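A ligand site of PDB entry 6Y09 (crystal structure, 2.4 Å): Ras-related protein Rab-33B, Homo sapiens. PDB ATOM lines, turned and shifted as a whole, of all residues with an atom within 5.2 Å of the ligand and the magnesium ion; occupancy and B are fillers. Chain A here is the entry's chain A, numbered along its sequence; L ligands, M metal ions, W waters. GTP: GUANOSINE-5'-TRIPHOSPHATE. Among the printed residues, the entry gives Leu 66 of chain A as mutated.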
ATOM      1  N   GLY A  14     -22.468  -1.955   9.573  1.00  0.00           N
ATOM      2  CA  GLY A  14     -21.461  -0.934   9.763  1.00  0.00           C
ATOM      3  C   GLY A  14     -20.673  -1.160  11.037  1.00  0.00           C
ATOM      4  O   GLY A  14     -20.957  -2.103  11.799  1.00  0.00           O
ATOM      5  N   ASP A  15     -19.674  -0.316  11.262  1.00  0.00           N
ATOM      6  CA  ASP A  15     -18.767  -0.438  12.399  1.00  0.00           C
ATOM      7  C   ASP A  15     -19.510  -0.378  13.727  1.00  0.00           C
ATOM      8  O   ASP A  15     -20.648   0.117  13.804  1.00  0.00           O
ATOM      9  CB  ASP A  15     -17.709   0.679  12.352  1.00  0.00           C
ATOM     10  CG  ASP A  15     -16.550   0.351  11.427  1.00  0.00           C
ATOM     11  OD1 ASP A  15     -16.639  -0.623  10.657  1.00  0.00           O
ATOM     12  OD2 ASP A  15     -15.528   1.092  11.479  1.00  0.00           O
ATOM     13  N   SER A  16     -18.881  -0.872  14.780  1.00  0.00           N
ATOM     14  CA  SER A  16     -19.465  -0.750  16.101  1.00  0.00           C
ATOM     15  C   SER A  16     -19.540   0.745  16.450  1.00  0.00           C
ATOM     16  O   SER A  16     -18.694   1.528  15.996  1.00  0.00           O
ATOM     17  CB  SER A  16     -18.645  -1.513  17.137  1.00  0.00           C
ATOM     18  OG  SER A  16     -19.246  -1.407  18.421  1.00  0.00           O
ATOM     19  N   ASN A  17     -20.558   1.122  17.218  1.00  0.00           N
ATOM     20  CA  ASN A  17     -20.737   2.500  17.725  1.00  0.00           C
ATOM     21  C   ASN A  17     -21.181   3.555  16.705  1.00  0.00           C
ATOM     22  O   ASN A  17     -21.147   4.738  17.013  1.00  0.00           O
ATOM     23  CB  ASN A  17     -19.452   2.996  18.378  1.00  0.00           C
ATOM     24  CG  ASN A  17     -19.493   2.839  19.862  1.00  0.00           C
ATOM     25  OD1 ASN A  17     -19.268   1.744  20.397  1.00  0.00           O
ATOM     26  ND2 ASN A  17     -19.785   3.937  20.561  1.00  0.00           N
ATOM     27  N   VAL A  18     -21.588   3.154  15.510  1.00  0.00           N
ATOM     28  CA  VAL A  18     -22.047   4.161  14.568  1.00  0.00           C
ATOM     29  C   VAL A  18     -23.521   4.466  14.834  1.00  0.00           C
ATOM     30  O   VAL A  18     -24.017   5.515  14.453  1.00  0.00           O
ATOM     31  CB  VAL A  18     -21.829   3.729  13.098  1.00  0.00           C
ATOM     32  CG1 VAL A  18     -20.366   3.424  12.859  1.00  0.00           C
ATOM     33  CG2 VAL A  18     -22.694   2.516  12.750  1.00  0.00           C
ATOM     34  N   GLY A  19     -24.197   3.547  15.521  1.00  0.00           N
ATOM     35  CA  GLY A  19     -25.569   3.786  15.955  1.00  0.00           C
ATOM     36  C   GLY A  19     -26.639   3.041  15.194  1.00  0.00           C
ATOM     37  O   GLY A  19     -27.762   3.531  15.035  1.00  0.00           O
ATOM     38  N   LYS A  20     -26.307   1.826  14.754  1.00  0.00           N
ATOM     39  CA  LYS A  20     -27.248   0.979  14.044  1.00  0.00           C
ATOM     40  C   LYS A  20     -28.432   0.609  14.944  1.00  0.00           C
ATOM     41  O   LYS A  20     -29.611   0.703  14.520  1.00  0.00           O
ATOM     42  CB  LYS A  20     -26.542  -0.280  13.535  1.00  0.00           C
ATOM     43  CG  LYS A  20     -25.242   0.019  12.770  1.00  0.00           C
ATOM     44  CD  LYS A  20     -24.586  -1.267  12.205  1.00  0.00           C
ATOM     45  CE  LYS A  20     -24.050  -2.186  13.290  1.00  0.00           C
ATOM     46  NZ  LYS A  20     -23.037  -1.506  14.158  1.00  0.00           N
ATOM     47  N   THR A  21     -28.142   0.194  16.185  1.00  0.00           N
ATOM     48  CA  THR A  21     -29.192  -0.129  17.145  1.00  0.00           C
ATOM     49  C   THR A  21     -30.100   1.078  17.378  1.00  0.00           C
ATOM     50  O   THR A  21     -31.327   0.951  17.300  1.00  0.00           O
ATOM     51  CB  THR A  21     -28.625  -0.604  18.492  1.00  0.00           C
ATOM     52  OG1 THR A  21     -27.907  -1.824  18.307  1.00  0.00           O
ATOM     53  CG2 THR A  21     -29.764  -0.811  19.516  1.00  0.00           C
ATOM     54  N   CYS A  22     -29.515   2.232  17.656  1.00  0.00           N
ATOM     55  CA  CYS A  22     -30.293   3.454  17.856  1.00  0.00           C
ATOM     56  C   CYS A  22     -31.142   3.869  16.643  1.00  0.00           C
ATOM     57  O   CYS A  22     -32.279   4.311  16.811  1.00  0.00           O
ATOM     58  CB  CYS A  22     -29.387   4.615  18.250  1.00  0.00           C
ATOM     59  SG  CYS A  22     -28.793   4.543  19.964  1.00  0.00           S
ATOM     60  N   PHE A  32     -35.692   7.077  21.346  1.00  0.00           N
ATOM     61  CA  PHE A  32     -34.262   6.824  21.488  1.00  0.00           C
ATOM     62  C   PHE A  32     -34.037   5.833  22.643  1.00  0.00           C
ATOM     63  O   PHE A  32     -34.725   5.917  23.658  1.00  0.00           O
ATOM     64  CB  PHE A  32     -33.511   8.139  21.746  1.00  0.00           C
ATOM     65  CG  PHE A  32     -32.034   8.068  21.473  1.00  0.00           C
ATOM     66  CD1 PHE A  32     -31.556   7.897  20.188  1.00  0.00           C
ATOM     67  CD2 PHE A  32     -31.122   8.213  22.506  1.00  0.00           C
ATOM     68  CE1 PHE A  32     -30.196   7.860  19.931  1.00  0.00           C
ATOM     69  CE2 PHE A  32     -29.757   8.164  22.267  1.00  0.00           C
ATOM     70  CZ  PHE A  32     -29.297   7.990  20.974  1.00  0.00           C
ATOM     71  N   THR A  36     -27.702   1.621  25.408  1.00  0.00           N
ATOM     72  CA  THR A  36     -27.290   0.582  24.469  1.00  0.00           C
ATOM     73  C   THR A  36     -26.036  -0.107  24.974  1.00  0.00           C
ATOM     74  O   THR A  36     -25.252   0.467  25.738  1.00  0.00           O
ATOM     75  CB  THR A  36     -27.011   1.128  23.030  1.00  0.00           C
ATOM     76  OG1 THR A  36     -26.223   2.327  23.106  1.00  0.00           O
ATOM     77  CG2 THR A  36     -28.310   1.416  22.287  1.00  0.00           C
ATOM     78  N   GLU A  37     -25.889  -1.356  24.577  1.00  0.00           N
ATOM     79  CA  GLU A  37     -24.659  -2.091  24.793  1.00  0.00           C
ATOM     80  C   GLU A  37     -24.356  -2.697  23.447  1.00  0.00           C
ATOM     81  O   GLU A  37     -25.227  -2.727  22.589  1.00  0.00           O
ATOM     82  CB  GLU A  37     -24.816  -3.185  25.846  1.00  0.00           C
ATOM     83  CG  GLU A  37     -25.502  -2.740  27.105  1.00  0.00           C
ATOM     84  CD  GLU A  37     -26.121  -3.901  27.837  1.00  0.00           C
ATOM     85  OE1 GLU A  37     -25.575  -4.302  28.888  1.00  0.00           O
ATOM     86  OE2 GLU A  37     -27.154  -4.422  27.348  1.00  0.00           O
ATOM     87  N   ALA A  38     -23.134  -3.189  23.266  1.00  0.00           N
ATOM     88  CA  ALA A  38     -22.715  -3.797  22.011  1.00  0.00           C
ATOM     89  C   ALA A  38     -23.704  -4.874  21.592  1.00  0.00           C
ATOM     90  O   ALA A  38     -24.033  -5.770  22.375  1.00  0.00           O
ATOM     91  CB  ALA A  38     -21.336  -4.374  22.140  1.00  0.00           C
ATOM     92  N   THR A  39     -24.227  -4.774  20.383  1.00  0.00           N
ATOM     93  CA  THR A  39     -25.117  -5.795  19.889  1.00  0.00           C
ATOM     94  C   THR A  39     -24.358  -7.111  19.704  1.00  0.00           C
ATOM     95  O   THR A  39     -23.256  -7.133  19.166  1.00  0.00           O
ATOM     96  CB  THR A  39     -25.769  -5.395  18.585  1.00  0.00           C
ATOM     97  OG1 THR A  39     -26.599  -4.247  18.826  1.00  0.00           O
ATOM     98  CG2 THR A  39     -26.626  -6.515  18.028  1.00  0.00           C
ATOM     99  N   ASP A  62     -30.702  -5.580  12.784  1.00  0.00           N
ATOM    100  CA  ASP A  62     -29.675  -4.736  13.383  1.00  0.00           C
ATOM    101  C   ASP A  62     -28.454  -5.612  13.656  1.00  0.00           C
ATOM    102  O   ASP A  62     -28.463  -6.356  14.661  1.00  0.00           O
ATOM    103  CB  ASP A  62     -30.256  -4.090  14.660  1.00  0.00           C
ATOM    104  CG  ASP A  62     -29.223  -3.374  15.496  1.00  0.00           C
ATOM    105  OD1 ASP A  62     -28.234  -2.867  14.930  1.00  0.00           O
ATOM    106  OD2 ASP A  62     -29.425  -3.303  16.730  1.00  0.00           O
ATOM    107  N   THR A  63     -27.442  -5.581  12.781  1.00  0.00           N
ATOM    108  CA  THR A  63     -26.362  -6.556  12.939  1.00  0.00           C
ATOM    109  C   THR A  63     -25.333  -6.055  13.949  1.00  0.00           C
ATOM    110  O   THR A  63     -25.401  -4.926  14.392  1.00  0.00           O
ATOM    111  CB  THR A  63     -25.591  -6.869  11.622  1.00  0.00           C
ATOM    112  OG1 THR A  63     -24.812  -5.743  11.210  1.00  0.00           O
ATOM    113  CG2 THR A  63     -26.515  -7.337  10.501  1.00  0.00           C
ATOM    114  N   ALA A  64     -24.381  -6.921  14.301  1.00  0.00           N
ATOM    115  CA  ALA A  64     -23.275  -6.504  15.158  1.00  0.00           C
ATOM    116  C   ALA A  64     -22.101  -5.962  14.329  1.00  0.00           C
ATOM    117  O   ALA A  64     -21.857  -6.402  13.211  1.00  0.00           O
ATOM    118  CB  ALA A  64     -22.820  -7.683  16.038  1.00  0.00           C
ATOM    119  N   GLY A  65     -21.375  -5.002  14.874  1.00  0.00           N
ATOM    120  CA  GLY A  65     -20.240  -4.431  14.167  1.00  0.00           C
ATOM    121  C   GLY A  65     -18.917  -4.951  14.676  1.00  0.00           C
ATOM    122  O   GLY A  65     -17.899  -4.806  14.038  1.00  0.00           O
ATOM    123  N   LEU A  66     -18.926  -5.540  15.870  1.00  0.00           N
ATOM    124  CA  LEU A  66     -17.708  -6.109  16.415  1.00  0.00           C
ATOM    125  C   LEU A  66     -17.425  -7.489  15.835  1.00  0.00           C
ATOM    126  O   LEU A  66     -18.328  -8.336  15.722  1.00  0.00           O
ATOM    127  CB  LEU A  66     -17.793  -6.177  17.936  1.00  0.00           C
ATOM    128  CG  LEU A  66     -17.699  -4.820  18.661  1.00  0.00           C
ATOM    129  CD1 LEU A  66     -18.056  -4.966  20.153  1.00  0.00           C
ATOM    130  CD2 LEU A  66     -16.294  -4.233  18.505  1.00  0.00           C
ATOM    131  N   ASN A 122     -24.661   8.836  10.242  1.00  0.00           N
ATOM    132  CA  ASN A 122     -25.405   9.064  11.478  1.00  0.00           C
ATOM    133  C   ASN A 122     -24.708  10.054  12.398  1.00  0.00           C
ATOM    134  O   ASN A 122     -23.500  10.293  12.249  1.00  0.00           O
ATOM    135  CB  ASN A 122     -25.597   7.744  12.230  1.00  0.00           C
ATOM    136  CG  ASN A 122     -26.598   7.871  13.375  1.00  0.00           C
ATOM    137  OD1 ASN A 122     -27.644   8.501  13.208  1.00  0.00           O
ATOM    138  ND2 ASN A 122     -26.268   7.308  14.548  1.00  0.00           N
ATOM    139  N   LYS A 123     -25.477  10.584  13.352  1.00  0.00           N
ATOM    140  CA  LYS A 123     -25.038  11.549  14.361  1.00  0.00           C
ATOM    141  C   LYS A 123     -24.759  12.922  13.734  1.00  0.00           C
ATOM    142  O   LYS A 123     -23.833  13.623  14.128  1.00  0.00           O
ATOM    143  CB  LYS A 123     -23.800  11.037  15.119  1.00  0.00           C
ATOM    144  CG  LYS A 123     -23.946   9.603  15.692  1.00  0.00           C
ATOM    145  CD  LYS A 123     -22.811   9.246  16.682  1.00  0.00           C
ATOM    146  CE  LYS A 123     -22.752   7.741  16.963  1.00  0.00           C
ATOM    147  NZ  LYS A 123     -21.576   7.326  17.802  1.00  0.00           N
ATOM    148  N   ASP A 125     -26.334  15.437  14.392  1.00  0.00           N
ATOM    149  CA  ASP A 125     -26.575  16.423  15.458  1.00  0.00           C
ATOM    150  C   ASP A 125     -25.291  16.884  16.150  1.00  0.00           C
ATOM    151  O   ASP A 125     -25.278  17.941  16.791  1.00  0.00           O
ATOM    152  CB  ASP A 125     -27.548  15.868  16.523  1.00  0.00           C
ATOM    153  CG  ASP A 125     -26.994  14.642  17.268  1.00  0.00           C
ATOM    154  OD1 ASP A 125     -27.016  13.524  16.691  1.00  0.00           O
ATOM    155  OD2 ASP A 125     -26.529  14.806  18.424  1.00  0.00           O
ATOM    156  N   LEU A 126     -24.223  16.120  16.038  1.00  0.00           N
ATOM    157  CA  LEU A 126     -22.946  16.487  16.659  1.00  0.00           C
ATOM    158  C   LEU A 126     -22.100  17.339  15.688  1.00  0.00           C
ATOM    159  O   LEU A 126     -20.958  16.993  15.370  1.00  0.00           O
ATOM    160  CB  LEU A 126     -22.170  15.233  17.086  1.00  0.00           C
ATOM    161  CG  LEU A 126     -22.881  14.292  18.063  1.00  0.00           C
ATOM    162  CD1 LEU A 126     -22.027  13.068  18.309  1.00  0.00           C
ATOM    163  CD2 LEU A 126     -23.222  14.987  19.401  1.00  0.00           C
ATOM    164  N   THR A 151     -28.208  11.731   8.837  1.00  0.00           N
ATOM    165  CA  THR A 151     -29.336  11.685   9.767  1.00  0.00           C
ATOM    166  C   THR A 151     -28.917  11.727  11.239  1.00  0.00           C
ATOM    167  O   THR A 151     -27.736  11.758  11.572  1.00  0.00           O
ATOM    168  CB  THR A 151     -30.191  10.412   9.521  1.00  0.00           C
ATOM    169  OG1 THR A 151     -31.446  10.505  10.190  1.00  0.00           O
ATOM    170  CG2 THR A 151     -29.457   9.172  10.024  1.00  0.00           C
ATOM    171  N   SER A 152     -29.900  11.742  12.141  1.00  0.00           N
ATOM    172  CA  SER A 152     -29.642  11.613  13.567  1.00  0.00           C
ATOM    173  C   SER A 152     -30.703  10.778  14.257  1.00  0.00           C
ATOM    174  O   SER A 152     -31.865  11.179  14.332  1.00  0.00           O
ATOM    175  CB  SER A 152     -29.562  12.982  14.271  1.00  0.00           C
ATOM    176  OG  SER A 152     -29.438  12.815  15.691  1.00  0.00           O
ATOM    177  N   ALA A 153     -30.301   9.633  14.791  1.00  0.00           N
ATOM    178  CA  ALA A 153     -31.236   8.795  15.515  1.00  0.00           C
ATOM    179  C   ALA A 153     -31.643   9.511  16.797  1.00  0.00           C
ATOM    180  O   ALA A 153     -32.765   9.354  17.290  1.00  0.00           O
ATOM    181  CB  ALA A 153     -30.611   7.433  15.801  1.00  0.00           C
ATOM    182  N   LYS A 154     -30.730  10.280  17.346  1.00  0.00           N
ATOM    183  CA  LYS A 154     -31.021  11.012  18.575  1.00  0.00           C
ATOM    184  C   LYS A 154     -32.044  12.130  18.317  1.00  0.00           C
ATOM    185  O   LYS A 154     -33.053  12.193  18.997  1.00  0.00           O
ATOM    186  CB  LYS A 154     -29.734  11.584  19.176  1.00  0.00           C
ATOM    187  CG  LYS A 154     -29.943  12.443  20.414  1.00  0.00           C
ATOM    188  CD  LYS A 154     -28.583  12.891  20.937  1.00  0.00           C
ATOM    189  CE  LYS A 154     -28.718  13.818  22.135  1.00  0.00           C
ATOM    190  NZ  LYS A 154     -29.671  13.241  23.125  1.00  0.00           N
ATOM    191  N   ASN A 155     -31.802  12.999  17.319  1.00  0.00           N
ATOM    192  CA  ASN A 155     -32.763  14.034  16.949  1.00  0.00           C
ATOM    193  C   ASN A 155     -33.381  13.759  15.574  1.00  0.00           C
ATOM    194  O   ASN A 155     -32.822  14.134  14.539  1.00  0.00           O
ATOM    195  CB  ASN A 155     -32.104  15.413  16.982  1.00  0.00           C
ATOM    196  CG  ASN A 155     -31.555  15.760  18.353  1.00  0.00           C
ATOM    197  OD1 ASN A 155     -32.095  15.330  19.380  1.00  0.00           O
ATOM    198  ND2 ASN A 155     -30.471  16.526  18.376  1.00  0.00           N
HETATM  199  PG  GTP L   1     -22.745  -2.124  17.816  1.00  0.00           P
HETATM  200  O1G GTP L   1     -22.461  -2.543  16.395  1.00  0.00           O
HETATM  201  O2G GTP L   1     -24.014  -2.761  18.328  1.00  0.00           O
HETATM  202  O3G GTP L   1     -21.581  -2.510  18.711  1.00  0.00           O
HETATM  203  O3B GTP L   1     -22.826  -0.511  17.876  1.00  0.00           O
HETATM  204  PB  GTP L   1     -24.073   0.325  17.289  1.00  0.00           P
HETATM  205  O1B GTP L   1     -23.807   0.671  15.846  1.00  0.00           O
HETATM  206  O2B GTP L   1     -25.407  -0.363  17.450  1.00  0.00           O
HETATM  207  O3A GTP L   1     -24.044   1.680  18.156  1.00  0.00           O
HETATM  208  PA  GTP L   1     -25.209   2.131  19.177  1.00  0.00           P
HETATM  209  O1A GTP L   1     -26.563   2.361  18.535  1.00  0.00           O
HETATM  210  O2A GTP L   1     -25.388   1.187  20.336  1.00  0.00           O
HETATM  211  O5' GTP L   1     -24.672   3.551  19.687  1.00  0.00           O
HETATM  212  C5' GTP L   1     -23.310   3.834  19.908  1.00  0.00           C
HETATM  213  C4' GTP L   1     -23.254   5.126  20.718  1.00  0.00           C
HETATM  214  O4' GTP L   1     -23.575   6.196  19.851  1.00  0.00           O
HETATM  215  C3' GTP L   1     -24.265   5.152  21.859  1.00  0.00           C
HETATM  216  O3' GTP L   1     -23.664   5.835  22.931  1.00  0.00           O
HETATM  217  C2' GTP L   1     -25.383   6.036  21.345  1.00  0.00           C
HETATM  218  O2' GTP L   1     -25.971   6.753  22.399  1.00  0.00           O
HETATM  219  C1' GTP L   1     -24.645   6.959  20.386  1.00  0.00           C
HETATM  220  N9  GTP L   1     -25.523   7.389  19.298  1.00  0.00           N
HETATM  221  C8  GTP L   1     -26.233   6.612  18.419  1.00  0.00           C
HETATM  222  N7  GTP L   1     -26.907   7.435  17.575  1.00  0.00           N
HETATM  223  C5  GTP L   1     -26.633   8.715  17.908  1.00  0.00           C
HETATM  224  C6  GTP L   1     -27.036   9.952  17.381  1.00  0.00           C
HETATM  225  O6  GTP L   1     -27.814  10.026  16.423  1.00  0.00           O
HETATM  226  N1  GTP L   1     -26.554  11.107  17.953  1.00  0.00           N
HETATM  227  C2  GTP L   1     -25.696  11.058  19.033  1.00  0.00           C
HETATM  228  N2  GTP L   1     -25.243  12.181  19.579  1.00  0.00           N
HETATM  229  N3  GTP L   1     -25.305   9.848  19.556  1.00  0.00           N
HETATM  230  C4  GTP L   1     -25.758   8.703  18.987  1.00  0.00           C
HETATM  231 MG    MG M   1     -25.932  -2.355  18.188  1.00  0.00          MG
HETATM  232  O   HOH W   1     -25.852  -1.604  20.264  1.00  0.00           O
HETATM  233  O   HOH W   2     -27.917   4.773  23.893  1.00  0.00           O
HETATM  234  O   HOH W   3     -23.632   0.429  22.180  1.00  0.00           O
HETATM  235  O   HOH W   4     -21.276  -5.404  18.201  1.00  0.00           O
HETATM  236  O   HOH W   5     -26.018  -3.063  16.344  1.00  0.00           O
HETATM  237  O   HOH W   6     -21.092  -0.619  20.854  1.00  0.00           O
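N of Thr 21 sits close to O2B of the ligand (3.1 Å).
An oxygen (O2G) of the ligand lies close to the backbone NH (N) of Thr 39 (2.9 Å).
The backbone NH (N) of Lys 20 sits at hydrogen-bond distance from an oxygen (O1B) of the ligand, at 3.0 Å.
O1G of the ligand lies within salt-bridge range of NZ of Lys 20 (2.5 Å).
The side-chain hydroxyl (OG) of Ser 16 is in hydrogen-bond range of an oxygen (O3G) of the ligand, at 2.6 Å.
The side-chain carboxylate (OD1) of Asp 125 is in hydrogen-bond range of a nitrogen (N1) of the ligand (2.8 Å).
The backbone NH (N) of Asn 17 lies within hydrogen-bond range of an oxygen (O3B) of the ligand.
An oxygen (O1B) of the ligand sits at hydrogen-bond distance from the backbone NH of Gly 19 (2.9 Å).
N of Ala 153 is in hydrogen-bond range of O6 of the ligand, 3.0 Å away.
N of Lys 154 lies within hydrogen-bond range of O6 of the ligand (3.1 Å).
The side-chain amino group (NZ) of Lys 123 is in hydrogen-bond range of an oxygen (O4') of the ligand, at 3.1 Å.
N of Cys 22 sits at hydrogen-bond distance from O1A of the ligand.
An oxygen (O1A) of the ligand sits at hydrogen-bond distance from the side-chain sulfur (SG) of Cys 22, at 3.4 Å.
The backbone NH (N) of Gly 65 is in hydrogen-bond range of an oxygen (O1G) of the ligand.
N7 of the ligand lies within hydrogen-bond range of ND2 of Asn 122 (3.1 Å).
An oxygen (O2A) of the ligand sits at hydrogen-bond distance from the side-chain hydroxyl (OG1) of Thr 36 (3.1 Å).
The side-chain hydroxyl (OG) of Ser 152 is in hydrogen-bond range of an oxygen (O6) of the ligand, 3.3 Å away.
The backbone NH (N) of Val 18 sits at hydrogen-bond distance from an oxygen (O1B) of the ligand, 3.3 Å away.
OD1 of Asp 62 lies within hydrogen-bond range of N of Thr 21 (3.3 Å).
The side-chain amino group (NZ) of Lys 20 is in hydrogen-bond range of the backbone carbonyl oxygen (O) of Asp 15 (2.9 Å).
The backbone carbonyl oxygen of Asn 17 lies within hydrogen-bond range of the side-chain amino group of Lys 123.
The side-chain amide oxygen (OD1) of Asn 122 lies within hydrogen-bond range of the backbone NH (N) of Ala 153 (3.3 Å).
N of Lys 154 sits close to OG of Ser 152 (3.3 Å).
The backbone NH of Lys 123 is in hydrogen-bond range of the backbone carbonyl oxygen of Thr 151, 3.1 Å away.
The backbone carbonyl oxygen (O) of Val 18 sits at hydrogen-bond distance from the side-chain amide nitrogen (ND2) of Asn 122 (2.9 Å).
The side-chain hydroxyl (OG) of Ser 152 is in hydrogen-bond range of the backbone NH (N) of Asn 155, 2.9 Å away.
Asp 15 touches the ligand (O to O1B, 3.8 Å).
Phe 32 touches the ligand (CZ to O2', 3.8 Å).
Ala 38 touches the ligand.
Leu 126 touches the ligand.
Hydrophobic or aromatic side chains within 4 Å of the ligand: Val 18, Phe 32, Ala 38, Leu 126 and Ala 153.
Along chain A the residues within 4 Å of the ligand span positions 15 to 154.
The nearest printed residue that does not touch the ligand is Ala 64 (4.01 Å).
OD2 of Asp 62 touches the magnesium ion (3.9 Å).
The nearest printed residue that does not touch the magnesium ion is Glu 37 (4.5 Å).
The magnesium ion is bound by O2G of the ligand (2.0 Å), water W5 (2.0 Å), OG1 of Thr 21 (2.0 Å), OG1 of Thr 39 (2.1 Å), O2B of the ligand (2.2 Å) and water W1 (2.2 Å).
Water W1 lies within hydrogen-bond range of O of Glu 37 (2.7 Å) and O2A of the ligand (2.8 Å).
Water W5 lies within hydrogen-bond range of the side-chain carboxylate of Asp 62 and the backbone carbonyl oxygen of Thr 63.
Water W3 lies within hydrogen-bond range of an oxygen (O2A) of the ligand and the side-chain hydroxyl of Thr 36.
Water W6 lies within hydrogen-bond range of an oxygen (O3G) of the ligand, the side-chain amide oxygen (OD1) of Asn 17 and the side-chain hydroxyl (OG) of Ser 16.
Water W4 lies within hydrogen-bond range of O of Thr 39 (2.8 Å), O3G of the ligand (3.0 Å), N of Leu 66 (3.3 Å) and N of Gly 65 (3.4 Å).
Water W2 bridges OG1 of Thr 36 (3.1 Å) and O2' of the ligand (3.2 Å).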
